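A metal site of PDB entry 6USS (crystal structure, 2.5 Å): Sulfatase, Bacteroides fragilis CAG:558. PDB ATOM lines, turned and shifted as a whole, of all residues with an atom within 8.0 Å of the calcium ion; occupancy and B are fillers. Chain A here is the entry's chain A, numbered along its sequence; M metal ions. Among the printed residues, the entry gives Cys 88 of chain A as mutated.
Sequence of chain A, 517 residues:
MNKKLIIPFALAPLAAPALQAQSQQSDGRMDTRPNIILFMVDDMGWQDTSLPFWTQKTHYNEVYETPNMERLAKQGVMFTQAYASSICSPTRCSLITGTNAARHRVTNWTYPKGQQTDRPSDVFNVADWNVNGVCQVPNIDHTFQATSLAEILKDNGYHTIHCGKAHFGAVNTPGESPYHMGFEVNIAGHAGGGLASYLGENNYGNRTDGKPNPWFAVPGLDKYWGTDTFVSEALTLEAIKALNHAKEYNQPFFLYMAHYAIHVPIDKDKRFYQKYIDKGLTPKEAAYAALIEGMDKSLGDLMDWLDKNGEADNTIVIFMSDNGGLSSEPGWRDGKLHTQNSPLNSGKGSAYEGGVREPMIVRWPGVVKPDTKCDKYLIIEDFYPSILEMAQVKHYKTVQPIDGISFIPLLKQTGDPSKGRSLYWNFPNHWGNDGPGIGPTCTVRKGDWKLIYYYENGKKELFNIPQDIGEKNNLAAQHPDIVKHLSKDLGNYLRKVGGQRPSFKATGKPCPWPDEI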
ATOM      1  N   MET A  40     -31.352  14.795   5.971  1.00  0.00           N
ATOM      2  CA  MET A  40     -29.907  14.626   5.851  1.00  0.00           C
ATOM      3  C   MET A  40     -29.514  13.267   6.410  1.00  0.00           C
ATOM      4  O   MET A  40     -29.720  12.996   7.611  1.00  0.00           O
ATOM      5  CB  MET A  40     -29.139  15.734   6.585  1.00  0.00           C
ATOM      6  CG  MET A  40     -27.630  15.630   6.473  1.00  0.00           C
ATOM      7  SD  MET A  40     -26.933  16.080   4.850  1.00  0.00           S
ATOM      8  CE  MET A  40     -27.514  17.774   4.721  1.00  0.00           C
ATOM      9  N   VAL A  41     -28.927  12.420   5.562  1.00  0.00           N
ATOM     10  CA  VAL A  41     -28.403  11.129   5.980  1.00  0.00           C
ATOM     11  C   VAL A  41     -26.910  11.258   6.226  1.00  0.00           C
ATOM     12  O   VAL A  41     -26.224  12.053   5.585  1.00  0.00           O
ATOM     13  CB  VAL A  41     -28.709  10.049   4.926  1.00  0.00           C
ATOM     14  CG1 VAL A  41     -28.357   8.682   5.465  1.00  0.00           C
ATOM     15  CG2 VAL A  41     -30.166  10.126   4.522  1.00  0.00           C
ATOM     16  N   ASP A  42     -26.408  10.480   7.181  1.00  0.00           N
ATOM     17  CA  ASP A  42     -24.996  10.521   7.546  1.00  0.00           C
ATOM     18  C   ASP A  42     -24.192   9.440   6.822  1.00  0.00           C
ATOM     19  O   ASP A  42     -24.599   8.274   6.802  1.00  0.00           O
ATOM     20  CB  ASP A  42     -24.841  10.341   9.058  1.00  0.00           C
ATOM     21  CG  ASP A  42     -23.486  10.738   9.537  1.00  0.00           C
ATOM     22  OD1 ASP A  42     -22.885  11.610   8.873  1.00  0.00           O
ATOM     23  OD2 ASP A  42     -23.006  10.200  10.556  1.00  0.00           O
ATOM     24  N   ASP A  43     -23.059   9.820   6.233  1.00  0.00           N
ATOM     25  CA  ASP A  43     -22.119   8.876   5.630  1.00  0.00           C
ATOM     26  C   ASP A  43     -22.773   8.004   4.557  1.00  0.00           C
ATOM     27  O   ASP A  43     -22.366   6.858   4.351  1.00  0.00           O
ATOM     28  CB  ASP A  43     -21.471   7.962   6.688  1.00  0.00           C
ATOM     29  CG  ASP A  43     -20.593   8.725   7.672  1.00  0.00           C
ATOM     30  OD1 ASP A  43     -20.322   9.917   7.397  1.00  0.00           O
ATOM     31  OD2 ASP A  43     -20.177   8.129   8.702  1.00  0.00           O
ATOM     32  N   MET A  44     -23.796   8.517   3.874  1.00  0.00           N
ATOM     33  CA  MET A  44     -24.465   7.783   2.810  1.00  0.00           C
ATOM     34  C   MET A  44     -23.773   8.047   1.465  1.00  0.00           C
ATOM     35  O   MET A  44     -23.579   9.208   1.092  1.00  0.00           O
ATOM     36  CB  MET A  44     -25.944   8.157   2.760  1.00  0.00           C
ATOM     37  CG  MET A  44     -26.742   7.517   1.632  1.00  0.00           C
ATOM     38  SD  MET A  44     -28.450   8.088   1.496  1.00  0.00           S
ATOM     39  CE  MET A  44     -29.022   7.162   0.058  1.00  0.00           C
ATOM     40  N   SER A  85     -18.318  18.061   1.671  1.00  0.00           N
ATOM     41  CA  SER A  85     -16.956  17.675   2.012  1.00  0.00           C
ATOM     42  C   SER A  85     -16.914  16.189   2.373  1.00  0.00           C
ATOM     43  O   SER A  85     -17.943  15.512   2.438  1.00  0.00           O
ATOM     44  CB  SER A  85     -16.385  18.529   3.155  1.00  0.00           C
ATOM     45  OG  SER A  85     -16.314  19.907   2.787  1.00  0.00           O
ATOM     46  N   SER A  86     -15.703  15.671   2.568  1.00  0.00           N
ATOM     47  CA  SER A  86     -15.550  14.229   2.743  1.00  0.00           C
ATOM     48  C   SER A  86     -15.737  13.772   4.181  1.00  0.00           C
ATOM     49  O   SER A  86     -15.660  12.568   4.441  1.00  0.00           O
ATOM     50  CB  SER A  86     -14.188  13.763   2.210  1.00  0.00           C
ATOM     51  OG  SER A  86     -13.121  14.344   2.930  1.00  0.00           O
ATOM     52  N   ILE A  87     -16.030  14.699   5.104  1.00  0.00           N
ATOM     53  CA  ILE A  87     -16.099  14.419   6.529  1.00  0.00           C
ATOM     54  C   ILE A  87     -17.247  15.229   7.114  1.00  0.00           C
ATOM     55  O   ILE A  87     -17.515  16.352   6.676  1.00  0.00           O
ATOM     56  CB  ILE A  87     -14.748  14.754   7.216  1.00  0.00           C
ATOM     57  CG1 ILE A  87     -13.714  13.700   6.866  1.00  0.00           C
ATOM     58  CG2 ILE A  87     -14.888  14.895   8.719  1.00  0.00           C
ATOM     59  CD1 ILE A  87     -14.075  12.310   7.337  1.00  0.00           C
ATOM     60  N   CYS A  88     -17.912  14.657   8.141  1.00  0.00           N
ATOM     61  CA  CYS A  88     -19.153  15.228   8.678  1.00  0.00           C
ATOM     62  C   CYS A  88     -19.014  16.700   9.062  1.00  0.00           C
ATOM     63  O   CYS A  88     -19.876  17.518   8.748  1.00  0.00           O
ATOM     64  CB  CYS A  88     -19.615  14.448   9.914  1.00  0.00           C
ATOM     65  SG  CYS A  88     -19.668  12.647   9.751  1.00  0.00           S
ATOM     66  N   SER A  89     -17.938  17.052   9.766  1.00  0.00           N
ATOM     67  CA  SER A  89     -17.895  18.377  10.389  1.00  0.00           C
ATOM     68  C   SER A  89     -17.790  19.502   9.369  1.00  0.00           C
ATOM     69  O   SER A  89     -18.578  20.459   9.454  1.00  0.00           O
ATOM     70  CB  SER A  89     -16.786  18.419  11.444  1.00  0.00           C
ATOM     71  OG  SER A  89     -17.178  17.755  12.625  1.00  0.00           O
ATOM     72  N   THR A  91     -18.770  19.562   6.304  1.00  0.00           N
ATOM     73  CA  THR A  91     -20.003  19.628   5.535  1.00  0.00           C
ATOM     74  C   THR A  91     -21.128  20.270   6.349  1.00  0.00           C
ATOM     75  O   THR A  91     -21.797  21.197   5.869  1.00  0.00           O
ATOM     76  CB  THR A  91     -20.415  18.233   5.068  1.00  0.00           C
ATOM     77  OG1 THR A  91     -19.448  17.764   4.124  1.00  0.00           O
ATOM     78  CG2 THR A  91     -21.793  18.259   4.418  1.00  0.00           C
ATOM     79  N   ARG A  92     -21.323  19.812   7.584  1.00  0.00           N
ATOM     80  CA  ARG A  92     -22.460  20.309   8.359  1.00  0.00           C
ATOM     81  C   ARG A  92     -22.282  21.770   8.738  1.00  0.00           C
ATOM     82  O   ARG A  92     -23.252  22.546   8.674  1.00  0.00           O
ATOM     83  CB  ARG A  92     -22.677  19.413   9.585  1.00  0.00           C
ATOM     84  CG  ARG A  92     -23.452  18.117   9.238  1.00  0.00           C
ATOM     85  CD  ARG A  92     -23.114  16.937  10.133  1.00  0.00           C
ATOM     86  NE  ARG A  92     -23.391  15.657   9.484  1.00  0.00           N
ATOM     87  CZ  ARG A  92     -24.594  15.100   9.387  1.00  0.00           C
ATOM     88  NH1 ARG A  92     -25.656  15.729   9.896  1.00  0.00           N
ATOM     89  NH2 ARG A  92     -24.742  13.926   8.775  1.00  0.00           N
ATOM     90  N   TRP A 109     -13.287  16.224  11.829  1.00  0.00           N
ATOM     91  CA  TRP A 109     -14.446  16.023  12.690  1.00  0.00           C
ATOM     92  C   TRP A 109     -14.196  16.458  14.141  1.00  0.00           C
ATOM     93  O   TRP A 109     -13.102  16.283  14.690  1.00  0.00           O
ATOM     94  CB  TRP A 109     -14.917  14.561  12.636  1.00  0.00           C
ATOM     95  CG  TRP A 109     -14.014  13.550  13.266  1.00  0.00           C
ATOM     96  CD1 TRP A 109     -13.013  12.862  12.650  1.00  0.00           C
ATOM     97  CD2 TRP A 109     -14.059  13.094  14.623  1.00  0.00           C
ATOM     98  NE1 TRP A 109     -12.420  11.999  13.555  1.00  0.00           N
ATOM     99  CE2 TRP A 109     -13.032  12.129  14.776  1.00  0.00           C
ATOM    100  CE3 TRP A 109     -14.858  13.411  15.731  1.00  0.00           C
ATOM    101  CZ2 TRP A 109     -12.790  11.483  15.992  1.00  0.00           C
ATOM    102  CZ3 TRP A 109     -14.616  12.761  16.938  1.00  0.00           C
ATOM    103  CH2 TRP A 109     -13.584  11.804  17.055  1.00  0.00           C
ATOM    104  N   LYS A 165     -28.677  14.061  14.356  1.00  0.00           N
ATOM    105  CA  LYS A 165     -27.276  14.438  14.478  1.00  0.00           C
ATOM    106  C   LYS A 165     -27.092  15.932  14.219  1.00  0.00           C
ATOM    107  O   LYS A 165     -27.389  16.421  13.129  1.00  0.00           O
ATOM    108  CB  LYS A 165     -26.424  13.623  13.508  1.00  0.00           C
ATOM    109  CG  LYS A 165     -25.081  14.236  13.189  1.00  0.00           C
ATOM    110  CD  LYS A 165     -24.105  13.155  12.761  1.00  0.00           C
ATOM    111  CE  LYS A 165     -22.864  13.760  12.139  1.00  0.00           C
ATOM    112  NZ  LYS A 165     -22.026  12.700  11.515  1.00  0.00           N
ATOM    113  N   HIS A 167     -23.936  17.989  15.667  1.00  0.00           N
ATOM    114  CA  HIS A 167     -22.502  17.937  15.391  1.00  0.00           C
ATOM    115  C   HIS A 167     -21.998  19.269  14.830  1.00  0.00           C
ATOM    116  O   HIS A 167     -21.255  19.311  13.846  1.00  0.00           O
ATOM    117  CB  HIS A 167     -22.224  16.759  14.439  1.00  0.00           C
ATOM    118  CG  HIS A 167     -20.791  16.340  14.376  1.00  0.00           C
ATOM    119  ND1 HIS A 167     -20.260  15.658  13.298  1.00  0.00           N
ATOM    120  CD2 HIS A 167     -19.775  16.493  15.265  1.00  0.00           C
ATOM    121  CE1 HIS A 167     -18.981  15.412  13.526  1.00  0.00           C
ATOM    122  NE2 HIS A 167     -18.659  15.901  14.710  1.00  0.00           N
ATOM    123  N   GLY A 193     -21.014  13.428  16.853  1.00  0.00           N
ATOM    124  CA  GLY A 193     -21.179  13.143  15.442  1.00  0.00           C
ATOM    125  C   GLY A 193     -21.451  11.680  15.168  1.00  0.00           C
ATOM    126  O   GLY A 193     -21.792  11.323  14.028  1.00  0.00           O
ATOM    127  N   HIS A 259     -30.411  12.252  10.226  1.00  0.00           N
ATOM    128  CA  HIS A 259     -30.293  10.903  10.783  1.00  0.00           C
ATOM    129  C   HIS A 259     -28.901  10.624  11.330  1.00  0.00           C
ATOM    130  O   HIS A 259     -27.893  11.163  10.846  1.00  0.00           O
ATOM    131  CB  HIS A 259     -30.641   9.860   9.713  1.00  0.00           C
ATOM    132  CG  HIS A 259     -32.090   9.575   9.627  1.00  0.00           C
ATOM    133  ND1 HIS A 259     -32.747   8.767  10.534  1.00  0.00           N
ATOM    134  CD2 HIS A 259     -33.045  10.028   8.777  1.00  0.00           C
ATOM    135  CE1 HIS A 259     -34.034   8.727  10.247  1.00  0.00           C
ATOM    136  NE2 HIS A 259     -34.241   9.477   9.174  1.00  0.00           N
ATOM    137  N   TYR A 260     -28.852   9.771  12.353  1.00  0.00           N
ATOM    138  CA  TYR A 260     -27.560   9.197  12.735  1.00  0.00           C
ATOM    139  C   TYR A 260     -27.160   8.070  11.789  1.00  0.00           C
ATOM    140  O   TYR A 260     -25.966   7.861  11.557  1.00  0.00           O
ATOM    141  CB  TYR A 260     -27.600   8.709  14.181  1.00  0.00           C
ATOM    142  CG  TYR A 260     -27.504   9.837  15.176  1.00  0.00           C
ATOM    143  CD1 TYR A 260     -26.283  10.393  15.479  1.00  0.00           C
ATOM    144  CD2 TYR A 260     -28.634  10.338  15.799  1.00  0.00           C
ATOM    145  CE1 TYR A 260     -26.181  11.434  16.368  1.00  0.00           C
ATOM    146  CE2 TYR A 260     -28.552  11.387  16.695  1.00  0.00           C
ATOM    147  CZ  TYR A 260     -27.310  11.932  16.982  1.00  0.00           C
ATOM    148  OH  TYR A 260     -27.180  12.975  17.894  1.00  0.00           O
ATOM    149  N   ALA A 261     -28.140   7.348  11.237  1.00  0.00           N
ATOM    150  CA  ALA A 261     -27.890   6.417  10.142  1.00  0.00           C
ATOM    151  C   ALA A 261     -27.285   7.175   8.964  1.00  0.00           C
ATOM    152  O   ALA A 261     -27.679   8.307   8.668  1.00  0.00           O
ATOM    153  CB  ALA A 261     -29.195   5.740   9.734  1.00  0.00           C
ATOM    154  N   ILE A 262     -26.324   6.555   8.275  1.00  0.00           N
ATOM    155  CA  ILE A 262     -25.973   5.155   8.396  1.00  0.00           C
ATOM    156  C   ILE A 262     -24.552   4.987   8.964  1.00  0.00           C
ATOM    157  O   ILE A 262     -23.760   4.184   8.462  1.00  0.00           O
ATOM    158  CB  ILE A 262     -26.110   4.457   7.043  1.00  0.00           C
ATOM    159  CG1 ILE A 262     -25.300   5.234   5.982  1.00  0.00           C
ATOM    160  CG2 ILE A 262     -27.583   4.360   6.666  1.00  0.00           C
ATOM    161  CD1 ILE A 262     -25.407   4.656   4.561  1.00  0.00           C
ATOM    162  N   HIS A 263     -24.256   5.784   9.991  1.00  0.00           N
ATOM    163  CA  HIS A 263     -22.952   5.845  10.625  1.00  0.00           C
ATOM    164  C   HIS A 263     -22.618   4.510  11.291  1.00  0.00           C
ATOM    165  O   HIS A 263     -23.495   3.715  11.624  1.00  0.00           O
ATOM    166  CB  HIS A 263     -22.954   6.973  11.671  1.00  0.00           C
ATOM    167  CG  HIS A 263     -21.591   7.459  12.050  1.00  0.00           C
ATOM    168  ND1 HIS A 263     -20.852   6.880  13.062  1.00  0.00           N
ATOM    169  CD2 HIS A 263     -20.830   8.456  11.546  1.00  0.00           C
ATOM    170  CE1 HIS A 263     -19.688   7.502  13.164  1.00  0.00           C
ATOM    171  NE2 HIS A 263     -19.647   8.468  12.260  1.00  0.00           N
ATOM    172  N   SER A 321     -27.049  13.876   1.612  1.00  0.00           N
ATOM    173  CA  SER A 321     -26.126  13.163   2.480  1.00  0.00           C
ATOM    174  C   SER A 321     -24.896  14.040   2.708  1.00  0.00           C
ATOM    175  O   SER A 321     -24.540  14.869   1.870  1.00  0.00           O
ATOM    176  CB  SER A 321     -25.719  11.803   1.897  1.00  0.00           C
ATOM    177  OG  SER A 321     -24.752  11.185   2.727  1.00  0.00           O
ATOM    178  N   ASP A 322     -24.224  13.818   3.833  1.00  0.00           N
ATOM    179  CA  ASP A 322     -23.171  14.732   4.246  1.00  0.00           C
ATOM    180  C   ASP A 322     -21.779  14.350   3.778  1.00  0.00           C
ATOM    181  O   ASP A 322     -20.884  15.196   3.835  1.00  0.00           O
ATOM    182  CB  ASP A 322     -23.169  14.884   5.780  1.00  0.00           C
ATOM    183  CG  ASP A 322     -22.542  13.699   6.472  1.00  0.00           C
ATOM    184  OD1 ASP A 322     -22.631  12.565   5.943  1.00  0.00           O
ATOM    185  OD2 ASP A 322     -21.934  13.909   7.540  1.00  0.00           O
ATOM    186  N   ASN A 323     -21.542  13.106   3.358  1.00  0.00           N
ATOM    187  CA  ASN A 323     -20.271  12.709   2.752  1.00  0.00           C
ATOM    188  C   ASN A 323     -20.403  11.284   2.209  1.00  0.00           C
ATOM    189  O   ASN A 323     -21.462  10.651   2.341  1.00  0.00           O
ATOM    190  CB  ASN A 323     -19.086  12.820   3.718  1.00  0.00           C
ATOM    191  CG  ASN A 323     -19.297  12.040   4.994  1.00  0.00           C
ATOM    192  OD1 ASN A 323     -19.361  10.797   4.984  1.00  0.00           O
ATOM    193  ND2 ASN A 323     -19.388  12.747   6.119  1.00  0.00           N
ATOM    194  N   GLY A 324     -19.324  10.786   1.594  1.00  0.00           N
ATOM    195  CA  GLY A 324     -19.363   9.479   0.963  1.00  0.00           C
ATOM    196  C   GLY A 324     -19.440   8.328   1.962  1.00  0.00           C
ATOM    197  O   GLY A 324     -19.147   8.465   3.157  1.00  0.00           O
ATOM    198  N   LYS A 348     -15.568   7.929   2.102  1.00  0.00           N
ATOM    199  CA  LYS A 348     -15.454   8.884   3.200  1.00  0.00           C
ATOM    200  C   LYS A 348     -13.998   9.185   3.527  1.00  0.00           C
ATOM    201  O   LYS A 348     -13.182   8.273   3.630  1.00  0.00           O
ATOM    202  CB  LYS A 348     -16.176   8.356   4.444  1.00  0.00           C
ATOM    203  CG  LYS A 348     -16.037   9.288   5.638  1.00  0.00           C
ATOM    204  CD  LYS A 348     -16.899   8.870   6.768  1.00  0.00           C
ATOM    205  CE  LYS A 348     -16.885   9.944   7.858  1.00  0.00           C
ATOM    206  NZ  LYS A 348     -17.798   9.612   8.952  1.00  0.00           N
ATOM    207  N   GLU A 358     -22.677  13.224  -3.455  1.00  0.00           N
ATOM    208  CA  GLU A 358     -23.777  12.860  -2.581  1.00  0.00           C
ATOM    209  C   GLU A 358     -25.099  12.690  -3.333  1.00  0.00           C
ATOM    210  O   GLU A 358     -25.349  13.374  -4.317  1.00  0.00           O
ATOM    211  CB  GLU A 358     -23.976  13.938  -1.500  1.00  0.00           C
ATOM    212  CG  GLU A 358     -22.742  14.222  -0.678  1.00  0.00           C
ATOM    213  CD  GLU A 358     -22.091  12.938  -0.194  1.00  0.00           C
ATOM    214  OE1 GLU A 358     -20.876  12.765  -0.461  1.00  0.00           O
ATOM    215  OE2 GLU A 358     -22.802  12.104   0.419  1.00  0.00           O
HETATM  216 CA    CA M   1     -20.791  12.050   8.034  1.00  0.00          CA
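The side-chain carboxylate (OE2) of Glu 358 sits close to the backbone NH (N) of Asn 323, at 3.4 Å.
OG of Ser 321 lies within hydrogen-bond range of O of Asn 323, 3.4 Å away.
The side-chain sulfur (SD) of Met 40 sits at hydrogen-bond distance from the backbone NH (N) of Asp 322 (3.7 Å).
The side-chain carboxylate (OD2) of Asp 322 sits close to the guanidinium group (NE) of Arg 92, 3.0 Å away.
NZ of Lys 165 is in hydrogen-bond range of O of Gly 193 (2.9 Å).
The guanidinium group of Arg 92 sits close to the side-chain carboxylate of Asp 42, at 3.0 Å.
The backbone carbonyl oxygen of Asp 322 sits at hydrogen-bond distance from the side-chain hydroxyl of Thr 91 (3.0 Å).
The backbone NH of Asp 42 sits at hydrogen-bond distance from the backbone carbonyl oxygen of Ala 261 (2.9 Å).
The calcium ion is bound by the side-chain sulfur (SG) of Cys 88 (2.1 Å), the side-chain carboxylate (OD2) of Asp 322 (2.2 Å), the side-chain carboxylate (OD1) of Asp 43 (2.3 Å), the side-chain carboxylate (OD1) of Asp 42 (2.3 Å), the side-chain amide nitrogen (ND2) of Asn 323 (2.5 Å) and the side-chain carboxylate (OD1) of Asp 322 (2.8 Å).
Residues that only touch the calcium ion: Lys 165 (3.8 Å) and Lys 348 (3.97 Å).
Of the 27 residues printed, 7 come within 4 Å of the calcium ion.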
